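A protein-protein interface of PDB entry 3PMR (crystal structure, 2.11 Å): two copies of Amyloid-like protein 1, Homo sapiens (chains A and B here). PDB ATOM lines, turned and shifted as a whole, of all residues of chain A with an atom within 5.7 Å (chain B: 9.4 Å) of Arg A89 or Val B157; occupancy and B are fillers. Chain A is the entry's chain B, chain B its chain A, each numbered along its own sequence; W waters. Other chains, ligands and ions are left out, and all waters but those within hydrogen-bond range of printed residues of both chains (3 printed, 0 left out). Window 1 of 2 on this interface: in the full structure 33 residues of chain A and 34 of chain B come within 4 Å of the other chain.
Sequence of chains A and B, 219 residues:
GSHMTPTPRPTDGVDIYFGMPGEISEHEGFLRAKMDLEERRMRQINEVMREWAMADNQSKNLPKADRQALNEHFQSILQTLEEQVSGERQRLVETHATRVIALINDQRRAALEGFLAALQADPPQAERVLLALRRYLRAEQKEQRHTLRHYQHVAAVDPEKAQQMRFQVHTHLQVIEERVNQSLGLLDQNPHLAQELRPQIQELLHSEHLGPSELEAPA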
ATOM      1  N   LYS A  34      -2.317  13.489  23.376  1.00  0.00           N
ATOM      2  CA  LYS A  34      -1.575  14.481  24.135  1.00  0.00           C
ATOM      3  C   LYS A  34      -0.148  14.657  23.583  1.00  0.00           C
ATOM      4  O   LYS A  34       0.343  15.780  23.477  1.00  0.00           O
ATOM      5  CB  LYS A  34      -1.556  14.070  25.611  1.00  0.00           C
ATOM      6  CG  LYS A  34      -0.945  15.082  26.548  1.00  0.00           C
ATOM      7  CD  LYS A  34      -1.156  14.677  28.014  1.00  0.00           C
ATOM      8  CE  LYS A  34      -0.268  15.511  28.939  1.00  0.00           C
ATOM      9  NZ  LYS A  34      -0.429  15.190  30.390  1.00  0.00           N
ATOM     10  N   GLU A  38       1.567  17.903  21.723  1.00  0.00           N
ATOM     11  CA  GLU A  38       2.768  18.431  22.364  1.00  0.00           C
ATOM     12  C   GLU A  38       3.795  18.730  21.275  1.00  0.00           C
ATOM     13  O   GLU A  38       4.383  19.813  21.225  1.00  0.00           O
ATOM     14  CB  GLU A  38       3.344  17.386  23.332  1.00  0.00           C
ATOM     15  CG  GLU A  38       4.681  17.773  23.963  1.00  0.00           C
ATOM     16  CD  GLU A  38       5.243  16.682  24.867  1.00  0.00           C
ATOM     17  OE1 GLU A  38       4.592  16.362  25.883  1.00  0.00           O
ATOM     18  OE2 GLU A  38       6.330  16.144  24.564  1.00  0.00           O
ATOM     19  N   GLN A  84      -4.139  29.232  22.314  1.00  0.00           N
ATOM     20  CA  GLN A  84      -4.550  28.048  21.579  1.00  0.00           C
ATOM     21  C   GLN A  84      -4.048  26.772  22.247  1.00  0.00           C
ATOM     22  O   GLN A  84      -4.752  25.767  22.260  1.00  0.00           O
ATOM     23  CB  GLN A  84      -4.023  28.099  20.145  1.00  0.00           C
ATOM     24  CG  GLN A  84      -4.704  29.141  19.281  1.00  0.00           C
ATOM     25  CD  GLN A  84      -4.215  29.102  17.853  1.00  0.00           C
ATOM     26  OE1 GLN A  84      -3.498  28.179  17.456  1.00  0.00           O
ATOM     27  NE2 GLN A  84      -4.609  30.096  17.062  1.00  0.00           N
ATOM     28  N   VAL A  85      -2.827  26.805  22.779  1.00  0.00           N
ATOM     29  CA  VAL A  85      -2.249  25.628  23.443  1.00  0.00           C
ATOM     30  C   VAL A  85      -3.083  25.290  24.686  1.00  0.00           C
ATOM     31  O   VAL A  85      -3.458  24.145  24.922  1.00  0.00           O
ATOM     32  CB  VAL A  85      -0.778  25.886  23.883  1.00  0.00           C
ATOM     33  CG1 VAL A  85      -0.264  24.701  24.705  1.00  0.00           C
ATOM     34  CG2 VAL A  85       0.114  26.110  22.647  1.00  0.00           C
ATOM     35  N   SER A  86      -3.344  26.318  25.475  1.00  0.00           N
ATOM     36  CA  SER A  86      -4.117  26.223  26.706  1.00  0.00           C
ATOM     37  C   SER A  86      -5.570  25.764  26.441  1.00  0.00           C
ATOM     38  O   SER A  86      -6.079  24.881  27.113  1.00  0.00           O
ATOM     39  CB  SER A  86      -4.090  27.602  27.373  1.00  0.00           C
ATOM     40  OG  SER A  86      -4.886  27.640  28.531  1.00  0.00           O
ATOM     41  N   GLY A  87      -6.222  26.375  25.455  1.00  0.00           N
ATOM     42  CA  GLY A  87      -7.598  26.020  25.135  1.00  0.00           C
ATOM     43  C   GLY A  87      -7.714  24.582  24.674  1.00  0.00           C
ATOM     44  O   GLY A  87      -8.690  23.886  24.968  1.00  0.00           O
ATOM     45  N   GLU A  88      -6.694  24.155  23.941  1.00  0.00           N
ATOM     46  CA  GLU A  88      -6.594  22.806  23.409  1.00  0.00           C
ATOM     47  C   GLU A  88      -6.398  21.764  24.523  1.00  0.00           C
ATOM     48  O   GLU A  88      -7.037  20.711  24.517  1.00  0.00           O
ATOM     49  CB  GLU A  88      -5.427  22.775  22.427  1.00  0.00           C
ATOM     50  CG  GLU A  88      -5.147  21.476  21.720  1.00  0.00           C
ATOM     51  CD  GLU A  88      -4.040  21.655  20.677  1.00  0.00           C
ATOM     52  OE1 GLU A  88      -2.923  22.083  21.053  1.00  0.00           O
ATOM     53  OE2 GLU A  88      -4.292  21.382  19.482  1.00  0.00           O
ATOM     54  N   ARG A  89      -5.517  22.044  25.476  1.00  0.00           N
ATOM     55  CA  ARG A  89      -5.293  21.092  26.565  1.00  0.00           C
ATOM     56  C   ARG A  89      -6.557  20.945  27.399  1.00  0.00           C
ATOM     57  O   ARG A  89      -6.892  19.864  27.858  1.00  0.00           O
ATOM     58  CB  ARG A  89      -4.167  21.570  27.479  1.00  0.00           C
ATOM     59  CG  ARG A  89      -3.960  20.700  28.737  1.00  0.00           C
ATOM     60  CD  ARG A  89      -3.637  19.248  28.370  1.00  0.00           C
ATOM     61  NE  ARG A  89      -2.399  19.123  27.599  1.00  0.00           N
ATOM     62  CZ  ARG A  89      -1.171  19.108  28.122  1.00  0.00           C
ATOM     63  NH1 ARG A  89      -0.995  19.207  29.438  1.00  0.00           N
ATOM     64  NH2 ARG A  89      -0.117  18.986  27.326  1.00  0.00           N
ATOM     65  N   GLN A  90      -7.243  22.060  27.592  1.00  0.00           N
ATOM     66  CA  GLN A  90      -8.455  22.101  28.388  1.00  0.00           C
ATOM     67  C   GLN A  90      -9.511  21.207  27.753  1.00  0.00           C
ATOM     68  O   GLN A  90     -10.245  20.505  28.445  1.00  0.00           O
ATOM     69  CB  GLN A  90      -8.950  23.540  28.469  1.00  0.00           C
ATOM     70  CG  GLN A  90      -9.889  23.822  29.609  1.00  0.00           C
ATOM     71  CD  GLN A  90     -10.166  25.304  29.759  1.00  0.00           C
ATOM     72  OE1 GLN A  90      -9.238  26.111  29.876  1.00  0.00           O
ATOM     73  NE2 GLN A  90     -11.444  25.673  29.759  1.00  0.00           N
ATOM     74  N   ARG A  91      -9.568  21.228  26.426  1.00  0.00           N
ATOM     75  CA  ARG A  91     -10.520  20.421  25.697  1.00  0.00           C
ATOM     76  C   ARG A  91     -10.150  18.936  25.782  1.00  0.00           C
ATOM     77  O   ARG A  91     -11.019  18.076  25.926  1.00  0.00           O
ATOM     78  CB  ARG A  91     -10.567  20.866  24.237  1.00  0.00           C
ATOM     79  CG  ARG A  91     -11.680  20.222  23.447  1.00  0.00           C
ATOM     80  CD  ARG A  91     -11.463  20.388  21.965  1.00  0.00           C
ATOM     81  NE  ARG A  91     -12.437  19.621  21.197  1.00  0.00           N
ATOM     82  CZ  ARG A  91     -12.312  19.347  19.902  1.00  0.00           C
ATOM     83  NH1 ARG A  91     -11.250  19.782  19.232  1.00  0.00           N
ATOM     84  NH2 ARG A  91     -13.239  18.630  19.280  1.00  0.00           N
ATOM     85  N   LEU A  92      -8.857  18.642  25.695  1.00  0.00           N
ATOM     86  CA  LEU A  92      -8.380  17.269  25.767  1.00  0.00           C
ATOM     87  C   LEU A  92      -8.638  16.675  27.158  1.00  0.00           C
ATOM     88  O   LEU A  92      -9.073  15.529  27.290  1.00  0.00           O
ATOM     89  CB  LEU A  92      -6.878  17.216  25.463  1.00  0.00           C
ATOM     90  CG  LEU A  92      -6.249  15.829  25.345  1.00  0.00           C
ATOM     91  CD1 LEU A  92      -6.716  15.159  24.059  1.00  0.00           C
ATOM     92  CD2 LEU A  92      -4.739  15.971  25.337  1.00  0.00           C
ATOM     93  N   VAL A  93      -8.366  17.466  28.185  1.00  0.00           N
ATOM     94  CA  VAL A  93      -8.560  17.033  29.562  1.00  0.00           C
ATOM     95  C   VAL A  93     -10.041  16.773  29.869  1.00  0.00           C
ATOM     96  O   VAL A  93     -10.381  15.776  30.501  1.00  0.00           O
ATOM     97  CB  VAL A  93      -8.001  18.096  30.542  1.00  0.00           C
ATOM     98  CG1 VAL A  93      -8.527  17.865  31.943  1.00  0.00           C
ATOM     99  CG2 VAL A  93      -6.479  18.039  30.538  1.00  0.00           C
ATOM    100  N   GLU A  94     -10.916  17.661  29.412  1.00  0.00           N
ATOM    101  CA  GLU A  94     -12.342  17.495  29.656  1.00  0.00           C
ATOM    102  C   GLU A  94     -12.894  16.252  28.966  1.00  0.00           C
ATOM    103  O   GLU A  94     -13.672  15.497  29.550  1.00  0.00           O
ATOM    104  CB  GLU A  94     -13.117  18.726  29.189  1.00  0.00           C
ATOM    105  CG  GLU A  94     -14.603  18.664  29.523  1.00  0.00           C
ATOM    106  N   ARG B 149       9.538  22.219  25.015  1.00  0.00           N
ATOM    107  CA  ARG B 149       8.547  21.461  25.759  1.00  0.00           C
ATOM    108  C   ARG B 149       8.176  22.116  27.091  1.00  0.00           C
ATOM    109  O   ARG B 149       7.009  22.112  27.483  1.00  0.00           O
ATOM    110  CB  ARG B 149       9.046  20.041  26.003  1.00  0.00           C
ATOM    111  CG  ARG B 149       8.012  19.150  26.667  1.00  0.00           C
ATOM    112  CD  ARG B 149       8.561  17.754  26.922  1.00  0.00           C
ATOM    113  NE  ARG B 149       8.943  17.065  25.689  1.00  0.00           N
ATOM    114  CZ  ARG B 149      10.197  16.899  25.275  1.00  0.00           C
ATOM    115  NH1 ARG B 149      11.213  17.374  25.991  1.00  0.00           N
ATOM    116  NH2 ARG B 149      10.442  16.244  24.149  1.00  0.00           N
ATOM    117  N   HIS B 150       9.165  22.667  27.786  1.00  0.00           N
ATOM    118  CA  HIS B 150       8.901  23.322  29.057  1.00  0.00           C
ATOM    119  C   HIS B 150       7.937  24.487  28.819  1.00  0.00           C
ATOM    120  O   HIS B 150       6.993  24.689  29.575  1.00  0.00           O
ATOM    121  CB  HIS B 150      10.192  23.855  29.674  1.00  0.00           C
ATOM    122  CG  HIS B 150       9.990  24.516  31.000  1.00  0.00           C
ATOM    123  ND1 HIS B 150      10.797  25.537  31.455  1.00  0.00           N
ATOM    124  CD2 HIS B 150       9.070  24.303  31.970  1.00  0.00           C
ATOM    125  CE1 HIS B 150      10.381  25.928  32.647  1.00  0.00           C
ATOM    126  NE2 HIS B 150       9.335  25.195  32.983  1.00  0.00           N
ATOM    127  N   TYR B 151       8.192  25.254  27.763  1.00  0.00           N
ATOM    128  CA  TYR B 151       7.341  26.390  27.418  1.00  0.00           C
ATOM    129  C   TYR B 151       5.939  25.919  27.022  1.00  0.00           C
ATOM    130  O   TYR B 151       4.936  26.479  27.471  1.00  0.00           O
ATOM    131  CB  TYR B 151       7.980  27.178  26.269  1.00  0.00           C
ATOM    132  CG  TYR B 151       7.191  28.384  25.794  1.00  0.00           C
ATOM    133  CD1 TYR B 151       6.596  29.269  26.701  1.00  0.00           C
ATOM    134  CD2 TYR B 151       7.080  28.665  24.432  1.00  0.00           C
ATOM    135  CE1 TYR B 151       5.908  30.406  26.253  1.00  0.00           C
ATOM    136  CE2 TYR B 151       6.401  29.792  23.977  1.00  0.00           C
ATOM    137  CZ  TYR B 151       5.821  30.651  24.884  1.00  0.00           C
ATOM    138  OH  TYR B 151       5.134  31.737  24.408  1.00  0.00           O
ATOM    139  N   GLN B 152       5.887  24.896  26.170  1.00  0.00           N
ATOM    140  CA  GLN B 152       4.628  24.335  25.708  1.00  0.00           C
ATOM    141  C   GLN B 152       3.778  23.850  26.882  1.00  0.00           C
ATOM    142  O   GLN B 152       2.556  24.035  26.894  1.00  0.00           O
ATOM    143  CB  GLN B 152       4.890  23.173  24.743  1.00  0.00           C
ATOM    144  CG  GLN B 152       3.657  22.299  24.450  1.00  0.00           C
ATOM    145  CD  GLN B 152       3.459  21.171  25.475  1.00  0.00           C
ATOM    146  OE1 GLN B 152       2.349  20.635  25.626  1.00  0.00           O
ATOM    147  NE2 GLN B 152       4.530  20.803  26.172  1.00  0.00           N
ATOM    148  N   HIS B 153       4.441  23.235  27.860  1.00  0.00           N
ATOM    149  CA  HIS B 153       3.788  22.702  29.052  1.00  0.00           C
ATOM    150  C   HIS B 153       3.201  23.781  29.934  1.00  0.00           C
ATOM    151  O   HIS B 153       2.083  23.636  30.425  1.00  0.00           O
ATOM    152  CB  HIS B 153       4.771  21.872  29.895  1.00  0.00           C
ATOM    153  CG  HIS B 153       4.166  21.323  31.151  1.00  0.00           C
ATOM    154  ND1 HIS B 153       3.439  20.152  31.173  1.00  0.00           N
ATOM    155  CD2 HIS B 153       4.141  21.805  32.417  1.00  0.00           C
ATOM    156  CE1 HIS B 153       2.992  19.937  32.399  1.00  0.00           C
ATOM    157  NE2 HIS B 153       3.403  20.926  33.172  1.00  0.00           N
ATOM    158  N   VAL B 154       3.971  24.839  30.167  1.00  0.00           N
ATOM    159  CA  VAL B 154       3.527  25.949  31.001  1.00  0.00           C
ATOM    160  C   VAL B 154       2.339  26.642  30.346  1.00  0.00           C
ATOM    161  O   VAL B 154       1.400  27.055  31.024  1.00  0.00           O
ATOM    162  CB  VAL B 154       4.650  26.987  31.220  1.00  0.00           C
ATOM    163  CG1 VAL B 154       4.099  28.201  31.959  1.00  0.00           C
ATOM    164  CG2 VAL B 154       5.790  26.363  32.019  1.00  0.00           C
ATOM    165  N   ALA B 155       2.382  26.760  29.024  1.00  0.00           N
ATOM    166  CA  ALA B 155       1.293  27.382  28.286  1.00  0.00           C
ATOM    167  C   ALA B 155       0.022  26.517  28.356  1.00  0.00           C
ATOM    168  O   ALA B 155      -1.090  27.031  28.477  1.00  0.00           O
ATOM    169  CB  ALA B 155       1.699  27.585  26.826  1.00  0.00           C
ATOM    170  N   ALA B 156       0.200  25.201  28.280  1.00  0.00           N
ATOM    171  CA  ALA B 156      -0.919  24.262  28.303  1.00  0.00           C
ATOM    172  C   ALA B 156      -1.655  24.199  29.628  1.00  0.00           C
ATOM    173  O   ALA B 156      -2.882  24.134  29.651  1.00  0.00           O
ATOM    174  CB  ALA B 156      -0.440  22.861  27.934  1.00  0.00           C
ATOM    175  N   VAL B 157      -0.918  24.222  30.731  1.00  0.00           N
ATOM    176  CA  VAL B 157      -1.551  24.108  32.035  1.00  0.00           C
ATOM    177  C   VAL B 157      -1.520  25.337  32.924  1.00  0.00           C
ATOM    178  O   VAL B 157      -2.121  25.334  33.996  1.00  0.00           O
ATOM    179  CB  VAL B 157      -0.942  22.945  32.829  1.00  0.00           C
ATOM    180  CG1 VAL B 157      -0.947  21.681  31.968  1.00  0.00           C
ATOM    181  CG2 VAL B 157       0.471  23.305  33.284  1.00  0.00           C
ATOM    182  N   ASP B 158      -0.819  26.380  32.501  1.00  0.00           N
ATOM    183  CA  ASP B 158      -0.746  27.601  33.305  1.00  0.00           C
ATOM    184  C   ASP B 158      -0.364  28.785  32.423  1.00  0.00           C
ATOM    185  O   ASP B 158       0.678  29.430  32.621  1.00  0.00           O
ATOM    186  CB  ASP B 158       0.268  27.417  34.436  1.00  0.00           C
ATOM    187  CG  ASP B 158       0.194  28.525  35.472  1.00  0.00           C
ATOM    188  OD1 ASP B 158      -0.823  29.256  35.497  1.00  0.00           O
ATOM    189  OD2 ASP B 158       1.146  28.658  36.268  1.00  0.00           O
ATOM    190  N   PRO B 159      -1.225  29.093  31.440  1.00  0.00           N
ATOM    191  CA  PRO B 159      -1.045  30.184  30.477  1.00  0.00           C
ATOM    192  C   PRO B 159      -0.705  31.555  31.061  1.00  0.00           C
ATOM    193  O   PRO B 159      -0.097  32.385  30.379  1.00  0.00           O
ATOM    194  CB  PRO B 159      -2.365  30.177  29.700  1.00  0.00           C
ATOM    195  CG  PRO B 159      -3.350  29.659  30.708  1.00  0.00           C
ATOM    196  CD  PRO B 159      -2.578  28.519  31.322  1.00  0.00           C
ATOM    197  N   GLU B 160      -1.079  31.793  32.315  1.00  0.00           N
ATOM    198  CA  GLU B 160      -0.799  33.082  32.945  1.00  0.00           C
ATOM    199  C   GLU B 160       0.702  33.318  33.089  1.00  0.00           C
ATOM    200  O   GLU B 160       1.197  34.417  32.841  1.00  0.00           O
ATOM    201  CB  GLU B 160      -1.462  33.155  34.323  1.00  0.00           C
ATOM    202  N   LYS B 161       1.417  32.270  33.477  1.00  0.00           N
ATOM    203  CA  LYS B 161       2.859  32.340  33.677  1.00  0.00           C
ATOM    204  C   LYS B 161       3.689  32.098  32.415  1.00  0.00           C
ATOM    205  O   LYS B 161       4.917  32.233  32.438  1.00  0.00           O
ATOM    206  CB  LYS B 161       3.276  31.331  34.741  1.00  0.00           C
ATOM    207  CG  LYS B 161       2.666  31.593  36.106  1.00  0.00           C
ATOM    208  N   ALA B 162       3.030  31.726  31.323  1.00  0.00           N
ATOM    209  CA  ALA B 162       3.740  31.477  30.078  1.00  0.00           C
ATOM    210  C   ALA B 162       4.341  32.766  29.521  1.00  0.00           C
ATOM    211  O   ALA B 162       5.478  32.772  29.045  1.00  0.00           O
ATOM    212  CB  ALA B 162       2.798  30.846  29.053  1.00  0.00           C
HETATM  213  O   HOH W   1      -5.562  23.940  29.680  1.00  0.00           O
HETATM  214  O   HOH W   2       8.020  15.519  22.645  1.00  0.00           O
HETATM  215  O   HOH W   3       0.835  20.864  23.316  1.00  0.00           O
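Water W2 bridges OE2 of Glu A38 and NH2 of Arg B149.
Water W1 lies within hydrogen-bond range of O of Ala B156, O of Ser A86 and N of Gln A90.
Water W3 lies within hydrogen-bond range of OE1 of Gln B152 and N of Glu A38.
The side-chain amide nitrogen (NE2) of Gln B152 sits at hydrogen-bond distance from the backbone carbonyl oxygen (O) of Arg B149.
Of the 14 printed residues of chain B, 6 touch a printed residue of chain A.
Hydrophobic or aromatic side chains of chain B within 4 Å of the printed part of chain A: Ala B156, Val B157 and Pro B159.
Among the printed residues, Asp or Glu carboxylates within 4 Å of a Lys or Arg side-chain nitrogen of the other chain: Glu A38 with Arg B149 (3.0 Å).
No position is printed for both chains.
Glu A38 touches Gln B152 (CG to NE2, 3.8 Å).
O of Gln B152 touches CG1 of Val A85, 3.6 Å away.
CG1 of Val A85 touches N of Ala B156 (3.6 Å).
Ser A86 touches Ala B155.
O of Ala B156 touches CA of Ser A86, at 3.8 Å.
OG of Ser A86 touches CG of Pro B159, 3.3 Å away.
CB of Arg A89 touches O of Ala B156, at 3.6 Å.
Arg A89 touches Val B157.
The guanidinium group (NE) of Arg B149 is in salt-bridge range of the side-chain carboxylate (OE2) of Glu A38 (3.0 Å).
OE1 of Gln B152 sits at hydrogen-bond distance from NH2 of Arg A89 (3.4 Å).
Of chain B, only Gln B152 (3.4 Å), Ala B156 (3.6 Å) and Val B157 (3.5 Å) come within 4 Å of Arg A89.
Of chain A, only Arg A89 comes within 4 Å of Val B157.
No residue of chain B comes within 4 Å of Gly A87.
Of the printed residues of chain A, Ala B155 touches Ser A86 (3.2 Å).
Of the printed residues of chain B, Glu A38 touches Arg B149 and Gln B152.
Printed residues of chain A within 4 Å of Pro B159: Ser A86.
Lys A34 touches none of the printed residues of chain B.
The nearest printed residue of chain B that does not touch Ser A86 is Val B157 (5.5 Å).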
